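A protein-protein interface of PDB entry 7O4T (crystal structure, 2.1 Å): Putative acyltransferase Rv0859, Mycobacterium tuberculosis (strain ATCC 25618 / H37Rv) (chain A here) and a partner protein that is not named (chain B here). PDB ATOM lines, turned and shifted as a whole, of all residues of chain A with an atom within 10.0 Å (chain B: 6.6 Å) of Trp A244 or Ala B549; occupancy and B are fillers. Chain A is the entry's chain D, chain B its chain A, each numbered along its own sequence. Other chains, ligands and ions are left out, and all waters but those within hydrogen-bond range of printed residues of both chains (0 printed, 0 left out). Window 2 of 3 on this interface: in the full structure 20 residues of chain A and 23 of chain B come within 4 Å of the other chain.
Among the printed residues, pairs that only touch across the chains: His A243 with Gln B553 (3.6 Å), Trp A244 with Ala B549 (3.7 Å) and Gln A240 with Gln B553 (3.8 Å).
Printed residues of chain B within 4 Å of Leu A239: Gln B553.
Printed residues of chain B within 4 Å of Gln A240: Gln B553.
Lys A241 touches none of the printed residues of chain B.
Of chain B, only Ala B549 (3.7 Å) and Ser B550 (3.3 Å) come within 4 Å of Trp A244.
Printed residues of chain B within 4 Å of Glu A246: Leu B631 (3.0 Å).
No residue of chain A comes within 4 Å of Pro B548.
Ala B549 touches two residues of chain A.
Of chain A, only His A243 and Trp A244 come within 4 Å of Ser B550.
Printed residues of chain A within 4 Å of Gln B553: Leu A239 (3.3 Å), Gln A240 (3.8 Å) and His A243 (3.6 Å).
Leu B565 touches none of the printed residues of chain A.
Of the printed residues of chain A, Leu B631 touches Glu A246 (3.0 Å).
The nearest printed residue of chain B that does not touch His A243 is Ile B551 (5.7 Å).
OG of Ser B550 sits at hydrogen-bond distance from ND1 of His A243 (2.7 Å).
N of Trp A244 lies close to OG of Ser B550, 3.4 Å away.
The side-chain amide nitrogen of Gln B553 sits at hydrogen-bond distance from the backbone carbonyl oxygen of Leu A239 (3.3 Å).
N of Leu B631 sits at hydrogen-bond distance from OE2 of Glu A246, at 3.0 Å.
The backbone carbonyl oxygen of His A243 sits close to the backbone carbonyl oxygen of Ala B549 (3.2 Å).
Hydrophobic or aromatic side chains of chain A that line the printed part of chain B: Leu A239, His A243 and Trp A244.
Among the printed residues, no Asp or Glu carboxylate lies within 4 Å of a Lys or Arg side-chain nitrogen of the other chain.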
ATOM      1  N   LEU A 155      -9.194  12.667  15.344  1.00  0.00           N
ATOM      2  CA  LEU A 155      -9.390  13.676  16.380  1.00  0.00           C
ATOM      3  C   LEU A 155      -9.176  15.083  15.832  1.00  0.00           C
ATOM      4  O   LEU A 155      -9.849  16.030  16.256  1.00  0.00           O
ATOM      5  CB  LEU A 155      -8.450  13.410  17.557  1.00  0.00           C
ATOM      6  CG  LEU A 155      -8.534  14.390  18.728  1.00  0.00           C
ATOM      7  CD1 LEU A 155      -9.909  14.334  19.374  1.00  0.00           C
ATOM      8  CD2 LEU A 155      -7.441  14.105  19.748  1.00  0.00           C
ATOM      9  N   ILE A 156      -8.242  15.241  14.891  1.00  0.00           N
ATOM     10  CA  ILE A 156      -8.005  16.552  14.290  1.00  0.00           C
ATOM     11  C   ILE A 156      -9.232  17.006  13.511  1.00  0.00           C
ATOM     12  O   ILE A 156      -9.691  18.147  13.645  1.00  0.00           O
ATOM     13  CB  ILE A 156      -6.749  16.517  13.402  1.00  0.00           C
ATOM     14  CG1 ILE A 156      -5.488  16.402  14.260  1.00  0.00           C
ATOM     15  CG2 ILE A 156      -6.682  17.755  12.521  1.00  0.00           C
ATOM     16  CD1 ILE A 156      -4.212  16.314  13.457  1.00  0.00           C
ATOM     17  N   THR A 158     -12.231  16.122  13.992  1.00  0.00           N
ATOM     18  CA  THR A 158     -13.310  16.391  14.936  1.00  0.00           C
ATOM     19  C   THR A 158     -13.178  17.783  15.543  1.00  0.00           C
ATOM     20  O   THR A 158     -14.157  18.534  15.620  1.00  0.00           O
ATOM     21  CB  THR A 158     -13.320  15.326  16.034  1.00  0.00           C
ATOM     22  OG1 THR A 158     -13.505  14.032  15.445  1.00  0.00           O
ATOM     23  CG2 THR A 158     -14.437  15.595  17.030  1.00  0.00           C
ATOM     24  N   ILE A 159     -11.971  18.144  15.979  1.00  0.00           N
ATOM     25  CA  ILE A 159     -11.767  19.437  16.625  1.00  0.00           C
ATOM     26  C   ILE A 159     -11.912  20.570  15.615  1.00  0.00           C
ATOM     27  O   ILE A 159     -12.615  21.558  15.861  1.00  0.00           O
ATOM     28  CB  ILE A 159     -10.396  19.478  17.322  1.00  0.00           C
ATOM     29  CG1 ILE A 159     -10.330  18.426  18.432  1.00  0.00           C
ATOM     30  CG2 ILE A 159     -10.116  20.870  17.874  1.00  0.00           C
ATOM     31  CD1 ILE A 159      -8.970  18.324  19.088  1.00  0.00           C
ATOM     32  N   GLU A 160     -11.253  20.445  14.462  1.00  0.00           N
ATOM     33  CA  GLU A 160     -11.255  21.516  13.474  1.00  0.00           C
ATOM     34  C   GLU A 160     -12.562  21.608  12.699  1.00  0.00           C
ATOM     35  O   GLU A 160     -12.859  22.669  12.139  1.00  0.00           O
ATOM     36  CB  GLU A 160     -10.092  21.332  12.499  1.00  0.00           C
ATOM     37  CG  GLU A 160      -8.720  21.384  13.157  1.00  0.00           C
ATOM     38  CD  GLU A 160      -8.383  22.760  13.703  1.00  0.00           C
ATOM     39  OE1 GLU A 160      -8.897  23.761  13.162  1.00  0.00           O
ATOM     40  OE2 GLU A 160      -7.601  22.840  14.674  1.00  0.00           O
ATOM     41  N   ALA A 238      -7.525   8.816  24.196  1.00  0.00           N
ATOM     42  CA  ALA A 238      -7.335  10.156  23.649  1.00  0.00           C
ATOM     43  C   ALA A 238      -8.273  11.161  24.302  1.00  0.00           C
ATOM     44  O   ALA A 238      -7.880  12.301  24.575  1.00  0.00           O
ATOM     45  CB  ALA A 238      -7.538  10.140  22.134  1.00  0.00           C
ATOM     46  N   LEU A 239      -9.519  10.757  24.570  1.00  0.00           N
ATOM     47  CA  LEU A 239     -10.484  11.686  25.142  1.00  0.00           C
ATOM     48  C   LEU A 239     -10.233  11.953  26.620  1.00  0.00           C
ATOM     49  O   LEU A 239     -10.773  12.925  27.158  1.00  0.00           O
ATOM     50  CB  LEU A 239     -11.904  11.163  24.930  1.00  0.00           C
ATOM     51  CG  LEU A 239     -12.354  11.156  23.466  1.00  0.00           C
ATOM     52  CD1 LEU A 239     -13.832  10.813  23.341  1.00  0.00           C
ATOM     53  CD2 LEU A 239     -12.052  12.495  22.807  1.00  0.00           C
ATOM     54  N   GLN A 240      -9.433  11.119  27.291  1.00  0.00           N
ATOM     55  CA  GLN A 240      -9.053  11.425  28.667  1.00  0.00           C
ATOM     56  C   GLN A 240      -8.159  12.658  28.736  1.00  0.00           C
ATOM     57  O   GLN A 240      -8.202  13.399  29.726  1.00  0.00           O
ATOM     58  CB  GLN A 240      -8.360  10.221  29.307  1.00  0.00           C
ATOM     59  CG  GLN A 240      -9.302   9.061  29.611  1.00  0.00           C
ATOM     60  CD  GLN A 240      -8.583   7.868  30.209  1.00  0.00           C
ATOM     61  OE1 GLN A 240      -7.495   8.001  30.771  1.00  0.00           O
ATOM     62  NE2 GLN A 240      -9.186   6.692  30.086  1.00  0.00           N
ATOM     63  N   LYS A 241      -7.349  12.897  27.704  1.00  0.00           N
ATOM     64  CA  LYS A 241      -6.563  14.123  27.622  1.00  0.00           C
ATOM     65  C   LYS A 241      -7.374  15.269  27.027  1.00  0.00           C
ATOM     66  O   LYS A 241      -7.417  16.365  27.595  1.00  0.00           O
ATOM     67  CB  LYS A 241      -5.292  13.896  26.801  1.00  0.00           C
ATOM     68  CG  LYS A 241      -4.569  15.190  26.458  1.00  0.00           C
ATOM     69  CD  LYS A 241      -3.067  15.069  26.630  1.00  0.00           C
ATOM     70  CE  LYS A 241      -2.408  16.438  26.564  1.00  0.00           C
ATOM     71  NZ  LYS A 241      -0.945  16.373  26.829  1.00  0.00           N
ATOM     72  N   TYR A 242      -8.019  15.031  25.885  1.00  0.00           N
ATOM     73  CA  TYR A 242      -8.903  16.023  25.270  1.00  0.00           C
ATOM     74  C   TYR A 242     -10.312  15.847  25.838  1.00  0.00           C
ATOM     75  O   TYR A 242     -11.251  15.419  25.165  1.00  0.00           O
ATOM     76  CB  TYR A 242      -8.873  15.891  23.753  1.00  0.00           C
ATOM     77  CG  TYR A 242      -7.531  16.235  23.146  1.00  0.00           C
ATOM     78  CD1 TYR A 242      -6.518  15.287  23.065  1.00  0.00           C
ATOM     79  CD2 TYR A 242      -7.276  17.510  22.656  1.00  0.00           C
ATOM     80  CE1 TYR A 242      -5.289  15.600  22.514  1.00  0.00           C
ATOM     81  CE2 TYR A 242      -6.051  17.831  22.103  1.00  0.00           C
ATOM     82  CZ  TYR A 242      -5.062  16.873  22.035  1.00  0.00           C
ATOM     83  OH  TYR A 242      -3.842  17.194  21.485  1.00  0.00           O
ATOM     84  N   HIS A 243     -10.439  16.203  27.119  1.00  0.00           N
ATOM     85  CA  HIS A 243     -11.648  15.891  27.870  1.00  0.00           C
ATOM     86  C   HIS A 243     -12.840  16.751  27.467  1.00  0.00           C
ATOM     87  O   HIS A 243     -13.980  16.376  27.762  1.00  0.00           O
ATOM     88  CB  HIS A 243     -11.379  16.028  29.369  1.00  0.00           C
ATOM     89  CG  HIS A 243     -10.683  17.297  29.750  1.00  0.00           C
ATOM     90  ND1 HIS A 243     -11.339  18.503  29.860  1.00  0.00           N
ATOM     91  CD2 HIS A 243      -9.388  17.543  30.062  1.00  0.00           C
ATOM     92  CE1 HIS A 243     -10.479  19.439  30.221  1.00  0.00           C
ATOM     93  NE2 HIS A 243      -9.289  18.883  30.350  1.00  0.00           N
ATOM     94  N   TRP A 244     -12.612  17.884  26.803  1.00  0.00           N
ATOM     95  CA  TRP A 244     -13.714  18.716  26.338  1.00  0.00           C
ATOM     96  C   TRP A 244     -14.328  18.213  25.040  1.00  0.00           C
ATOM     97  O   TRP A 244     -15.348  18.758  24.605  1.00  0.00           O
ATOM     98  CB  TRP A 244     -13.245  20.161  26.155  1.00  0.00           C
ATOM     99  CG  TRP A 244     -12.193  20.315  25.102  1.00  0.00           C
ATOM    100  CD1 TRP A 244     -12.388  20.621  23.788  1.00  0.00           C
ATOM    101  CD2 TRP A 244     -10.779  20.163  25.274  1.00  0.00           C
ATOM    102  NE1 TRP A 244     -11.183  20.672  23.130  1.00  0.00           N
ATOM    103  CE2 TRP A 244     -10.179  20.395  24.020  1.00  0.00           C
ATOM    104  CE3 TRP A 244      -9.961  19.855  26.366  1.00  0.00           C
ATOM    105  CZ2 TRP A 244      -8.800  20.329  23.828  1.00  0.00           C
ATOM    106  CZ3 TRP A 244      -8.593  19.790  26.173  1.00  0.00           C
ATOM    107  CH2 TRP A 244      -8.027  20.026  24.914  1.00  0.00           C
ATOM    108  N   VAL A 245     -13.738  17.201  24.412  1.00  0.00           N
ATOM    109  CA  VAL A 245     -14.284  16.588  23.208  1.00  0.00           C
ATOM    110  C   VAL A 245     -15.092  15.366  23.629  1.00  0.00           C
ATOM    111  O   VAL A 245     -14.559  14.448  24.264  1.00  0.00           O
ATOM    112  CB  VAL A 245     -13.175  16.205  22.216  1.00  0.00           C
ATOM    113  CG1 VAL A 245     -13.770  15.538  20.988  1.00  0.00           C
ATOM    114  CG2 VAL A 245     -12.368  17.438  21.824  1.00  0.00           C
ATOM    115  N   GLU A 246     -16.377  15.355  23.275  1.00  0.00           N
ATOM    116  CA  GLU A 246     -17.263  14.277  23.703  1.00  0.00           C
ATOM    117  C   GLU A 246     -17.075  13.023  22.856  1.00  0.00           C
ATOM    118  O   GLU A 246     -16.974  11.914  23.392  1.00  0.00           O
ATOM    119  CB  GLU A 246     -18.719  14.745  23.645  1.00  0.00           C
ATOM    120  CG  GLU A 246     -19.734  13.668  23.981  1.00  0.00           C
ATOM    121  CD  GLU A 246     -21.166  14.120  23.755  1.00  0.00           C
ATOM    122  OE1 GLU A 246     -21.368  15.265  23.296  1.00  0.00           O
ATOM    123  OE2 GLU A 246     -22.088  13.326  24.034  1.00  0.00           O
ATOM    124  N   LYS A 247     -17.023  13.179  21.535  1.00  0.00           N
ATOM    125  CA  LYS A 247     -17.017  12.053  20.615  1.00  0.00           C
ATOM    126  C   LYS A 247     -16.042  12.329  19.479  1.00  0.00           C
ATOM    127  O   LYS A 247     -15.925  13.467  19.017  1.00  0.00           O
ATOM    128  CB  LYS A 247     -18.426  11.799  20.054  1.00  0.00           C
ATOM    129  CG  LYS A 247     -18.516  10.681  19.025  1.00  0.00           C
ATOM    130  CD  LYS A 247     -18.848   9.348  19.673  1.00  0.00           C
ATOM    131  CE  LYS A 247     -20.256   8.899  19.309  1.00  0.00           C
ATOM    132  NZ  LYS A 247     -20.414   8.707  17.840  1.00  0.00           N
ATOM    133  N   ILE A 248     -15.350  11.283  19.031  1.00  0.00           N
ATOM    134  CA  ILE A 248     -14.420  11.373  17.909  1.00  0.00           C
ATOM    135  C   ILE A 248     -15.138  10.933  16.642  1.00  0.00           C
ATOM    136  O   ILE A 248     -15.712   9.837  16.592  1.00  0.00           O
ATOM    137  CB  ILE A 248     -13.163  10.519  18.152  1.00  0.00           C
ATOM    138  CG1 ILE A 248     -12.320  11.117  19.281  1.00  0.00           C
ATOM    139  CG2 ILE A 248     -12.348  10.398  16.874  1.00  0.00           C
ATOM    140  CD1 ILE A 248     -11.071  10.321  19.593  1.00  0.00           C
ATOM    141  N   ASP A 295       1.612  17.999  20.638  1.00  0.00           N
ATOM    142  CA  ASP A 295       1.077  16.997  21.553  1.00  0.00           C
ATOM    143  C   ASP A 295       1.217  15.597  20.961  1.00  0.00           C
ATOM    144  O   ASP A 295       0.868  15.385  19.791  1.00  0.00           O
ATOM    145  CB  ASP A 295      -0.390  17.291  21.865  1.00  0.00           C
ATOM    146  CG  ASP A 295      -1.004  16.266  22.799  1.00  0.00           C
ATOM    147  OD1 ASP A 295      -0.558  16.178  23.963  1.00  0.00           O
ATOM    148  OD2 ASP A 295      -1.933  15.548  22.371  1.00  0.00           O
ATOM    149  N   VAL A 297      -0.428  12.790  21.749  1.00  0.00           N
ATOM    150  CA  VAL A 297      -1.677  12.050  21.597  1.00  0.00           C
ATOM    151  C   VAL A 297      -2.334  12.389  20.264  1.00  0.00           C
ATOM    152  O   VAL A 297      -2.706  11.498  19.491  1.00  0.00           O
ATOM    153  CB  VAL A 297      -2.618  12.328  22.781  1.00  0.00           C
ATOM    154  CG1 VAL A 297      -3.912  11.543  22.620  1.00  0.00           C
ATOM    155  CG2 VAL A 297      -1.933  11.977  24.093  1.00  0.00           C
ATOM    156  N   ILE A 298      -2.488  13.684  19.974  1.00  0.00           N
ATOM    157  CA  ILE A 298      -2.964  14.089  18.655  1.00  0.00           C
ATOM    158  C   ILE A 298      -1.888  13.822  17.609  1.00  0.00           C
ATOM    159  O   ILE A 298      -2.197  13.594  16.432  1.00  0.00           O
ATOM    160  CB  ILE A 298      -3.407  15.565  18.681  1.00  0.00           C
ATOM    161  CG1 ILE A 298      -4.632  15.777  17.791  1.00  0.00           C
ATOM    162  CG2 ILE A 298      -2.281  16.493  18.254  1.00  0.00           C
ATOM    163  CD1 ILE A 298      -5.168  17.195  17.830  1.00  0.00           C
ATOM    164  N   VAL B 546     -18.374  25.446  32.390  1.00  0.00           N
ATOM    165  CA  VAL B 546     -17.458  24.360  32.064  1.00  0.00           C
ATOM    166  C   VAL B 546     -18.112  23.426  31.056  1.00  0.00           C
ATOM    167  O   VAL B 546     -19.311  23.126  31.145  1.00  0.00           O
ATOM    168  CB  VAL B 546     -17.048  23.608  33.343  1.00  0.00           C
ATOM    169  CG1 VAL B 546     -16.077  22.485  33.018  1.00  0.00           C
ATOM    170  CG2 VAL B 546     -16.439  24.571  34.348  1.00  0.00           C
ATOM    171  N   GLU B 547     -17.325  22.972  30.083  1.00  0.00           N
ATOM    172  CA  GLU B 547     -17.822  22.036  29.082  1.00  0.00           C
ATOM    173  C   GLU B 547     -18.409  20.802  29.761  1.00  0.00           C
ATOM    174  O   GLU B 547     -17.758  20.214  30.635  1.00  0.00           O
ATOM    175  CB  GLU B 547     -16.697  21.621  28.134  1.00  0.00           C
ATOM    176  CG  GLU B 547     -16.178  22.734  27.236  1.00  0.00           C
ATOM    177  CD  GLU B 547     -17.015  22.913  25.982  1.00  0.00           C
ATOM    178  OE1 GLU B 547     -18.037  22.209  25.837  1.00  0.00           O
ATOM    179  OE2 GLU B 547     -16.646  23.755  25.138  1.00  0.00           O
ATOM    180  N   PRO B 548     -19.624  20.382  29.397  1.00  0.00           N
ATOM    181  CA  PRO B 548     -20.199  19.187  30.033  1.00  0.00           C
ATOM    182  C   PRO B 548     -19.398  17.926  29.770  1.00  0.00           C
ATOM    183  O   PRO B 548     -19.403  17.015  30.607  1.00  0.00           O
ATOM    184  CB  PRO B 548     -21.607  19.108  29.423  1.00  0.00           C
ATOM    185  CG  PRO B 548     -21.517  19.873  28.146  1.00  0.00           C
ATOM    186  CD  PRO B 548     -20.532  20.975  28.401  1.00  0.00           C
ATOM    187  N   ALA B 549     -18.702  17.846  28.633  1.00  0.00           N
ATOM    188  CA  ALA B 549     -17.850  16.690  28.374  1.00  0.00           C
ATOM    189  C   ALA B 549     -16.700  16.623  29.370  1.00  0.00           C
ATOM    190  O   ALA B 549     -16.298  15.533  29.795  1.00  0.00           O
ATOM    191  CB  ALA B 549     -17.317  16.736  26.942  1.00  0.00           C
ATOM    192  N   SER B 550     -16.156  17.781  29.755  1.00  0.00           N
ATOM    193  CA  SER B 550     -15.084  17.799  30.743  1.00  0.00           C
ATOM    194  C   SER B 550     -15.604  17.435  32.126  1.00  0.00           C
ATOM    195  O   SER B 550     -14.908  16.772  32.903  1.00  0.00           O
ATOM    196  CB  SER B 550     -14.415  19.174  30.768  1.00  0.00           C
ATOM    197  OG  SER B 550     -13.828  19.479  29.515  1.00  0.00           O
ATOM    198  N   ILE B 551     -16.827  17.864  32.450  1.00  0.00           N
ATOM    199  CA  ILE B 551     -17.420  17.530  33.743  1.00  0.00           C
ATOM    200  C   ILE B 551     -17.583  16.021  33.877  1.00  0.00           C
ATOM    201  O   ILE B 551     -17.260  15.433  34.917  1.00  0.00           O
ATOM    202  CB  ILE B 551     -18.762  18.262  33.922  1.00  0.00           C
ATOM    203  CG1 ILE B 551     -18.541  19.775  33.953  1.00  0.00           C
ATOM    204  CG2 ILE B 551     -19.469  17.792  35.186  1.00  0.00           C
ATOM    205  CD1 ILE B 551     -19.822  20.573  34.024  1.00  0.00           C
ATOM    206  N   GLU B 552     -18.087  15.372  32.824  1.00  0.00           N
ATOM    207  CA  GLU B 552     -18.229  13.919  32.855  1.00  0.00           C
ATOM    208  C   GLU B 552     -16.868  13.234  32.884  1.00  0.00           C
ATOM    209  O   GLU B 552     -16.698  12.208  33.556  1.00  0.00           O
ATOM    210  CB  GLU B 552     -19.048  13.444  31.656  1.00  0.00           C
ATOM    211  CG  GLU B 552     -20.448  14.047  31.563  1.00  0.00           C
ATOM    212  CD  GLU B 552     -21.374  13.586  32.677  1.00  0.00           C
ATOM    213  OE1 GLU B 552     -21.179  14.001  33.839  1.00  0.00           O
ATOM    214  OE2 GLU B 552     -22.302  12.800  32.390  1.00  0.00           O
ATOM    215  N   GLN B 553     -15.886  13.785  32.166  1.00  0.00           N
ATOM    216  CA  GLN B 553     -14.539  13.225  32.206  1.00  0.00           C
ATOM    217  C   GLN B 553     -13.928  13.356  33.593  1.00  0.00           C
ATOM    218  O   GLN B 553     -13.229  12.450  34.060  1.00  0.00           O
ATOM    219  CB  GLN B 553     -13.650  13.908  31.166  1.00  0.00           C
ATOM    220  CG  GLN B 553     -13.770  13.332  29.763  1.00  0.00           C
ATOM    221  CD  GLN B 553     -13.110  11.971  29.628  1.00  0.00           C
ATOM    222  OE1 GLN B 553     -12.398  11.520  30.526  1.00  0.00           O
ATOM    223  NE2 GLN B 553     -13.344  11.311  28.500  1.00  0.00           N
ATOM    224  N   ALA B 554     -14.179  14.480  34.270  1.00  0.00           N
ATOM    225  CA  ALA B 554     -13.637  14.668  35.611  1.00  0.00           C
ATOM    226  C   ALA B 554     -14.238  13.674  36.595  1.00  0.00           C
ATOM    227  O   ALA B 554     -13.546  13.189  37.499  1.00  0.00           O
ATOM    228  CB  ALA B 554     -13.878  16.102  36.080  1.00  0.00           C
ATOM    229  N   LEU B 565     -23.341  14.118  35.651  1.00  0.00           N
ATOM    230  CA  LEU B 565     -24.519  14.544  34.897  1.00  0.00           C
ATOM    231  C   LEU B 565     -25.386  13.349  34.517  1.00  0.00           C
ATOM    232  O   LEU B 565     -26.619  13.427  34.569  1.00  0.00           O
ATOM    233  CB  LEU B 565     -24.106  15.326  33.650  1.00  0.00           C
ATOM    234  CG  LEU B 565     -23.306  16.611  33.876  1.00  0.00           C
ATOM    235  CD1 LEU B 565     -23.143  17.374  32.571  1.00  0.00           C
ATOM    236  CD2 LEU B 565     -23.964  17.482  34.931  1.00  0.00           C
ATOM    237  N   LEU B 631     -24.866  13.765  25.097  1.00  0.00           N
ATOM    238  CA  LEU B 631     -25.168  15.032  25.749  1.00  0.00           C
ATOM    239  C   LEU B 631     -26.067  15.885  24.863  1.00  0.00           C
ATOM    240  O   LEU B 631     -25.912  15.919  23.638  1.00  0.00           O
ATOM    241  CB  LEU B 631     -23.879  15.784  26.078  1.00  0.00           C
ATOM    242  CG  LEU B 631     -23.046  15.223  27.231  1.00  0.00           C
ATOM    243  CD1 LEU B 631     -21.733  15.972  27.355  1.00  0.00           C
ATOM    244  CD2 LEU B 631     -23.828  15.294  28.532  1.00  0.00           C
ATOM    245  N   ARG B 636     -24.785  23.394  25.595  1.00  0.00           N
ATOM    246  CA  ARG B 636     -23.683  24.344  25.483  1.00  0.00           C
ATOM    247  C   ARG B 636     -24.178  25.763  25.234  1.00  0.00           C
ATOM    248  O   ARG B 636     -23.536  26.726  25.667  1.00  0.00           O
ATOM    249  CB  ARG B 636     -22.726  23.905  24.374  1.00  0.00           C
ATOM    250  CG  ARG B 636     -22.135  22.517  24.593  1.00  0.00           C
ATOM    251  CD  ARG B 636     -21.201  22.101  23.466  1.00  0.00           C
ATOM    252  NE  ARG B 636     -19.928  22.818  23.501  1.00  0.00           N
ATOM    253  CZ  ARG B 636     -19.643  23.879  22.752  1.00  0.00           C
ATOM    254  NH1 ARG B 636     -20.541  24.356  21.901  1.00  0.00           N
ATOM    255  NH2 ARG B 636     -18.457  24.463  22.853  1.00  0.00           N
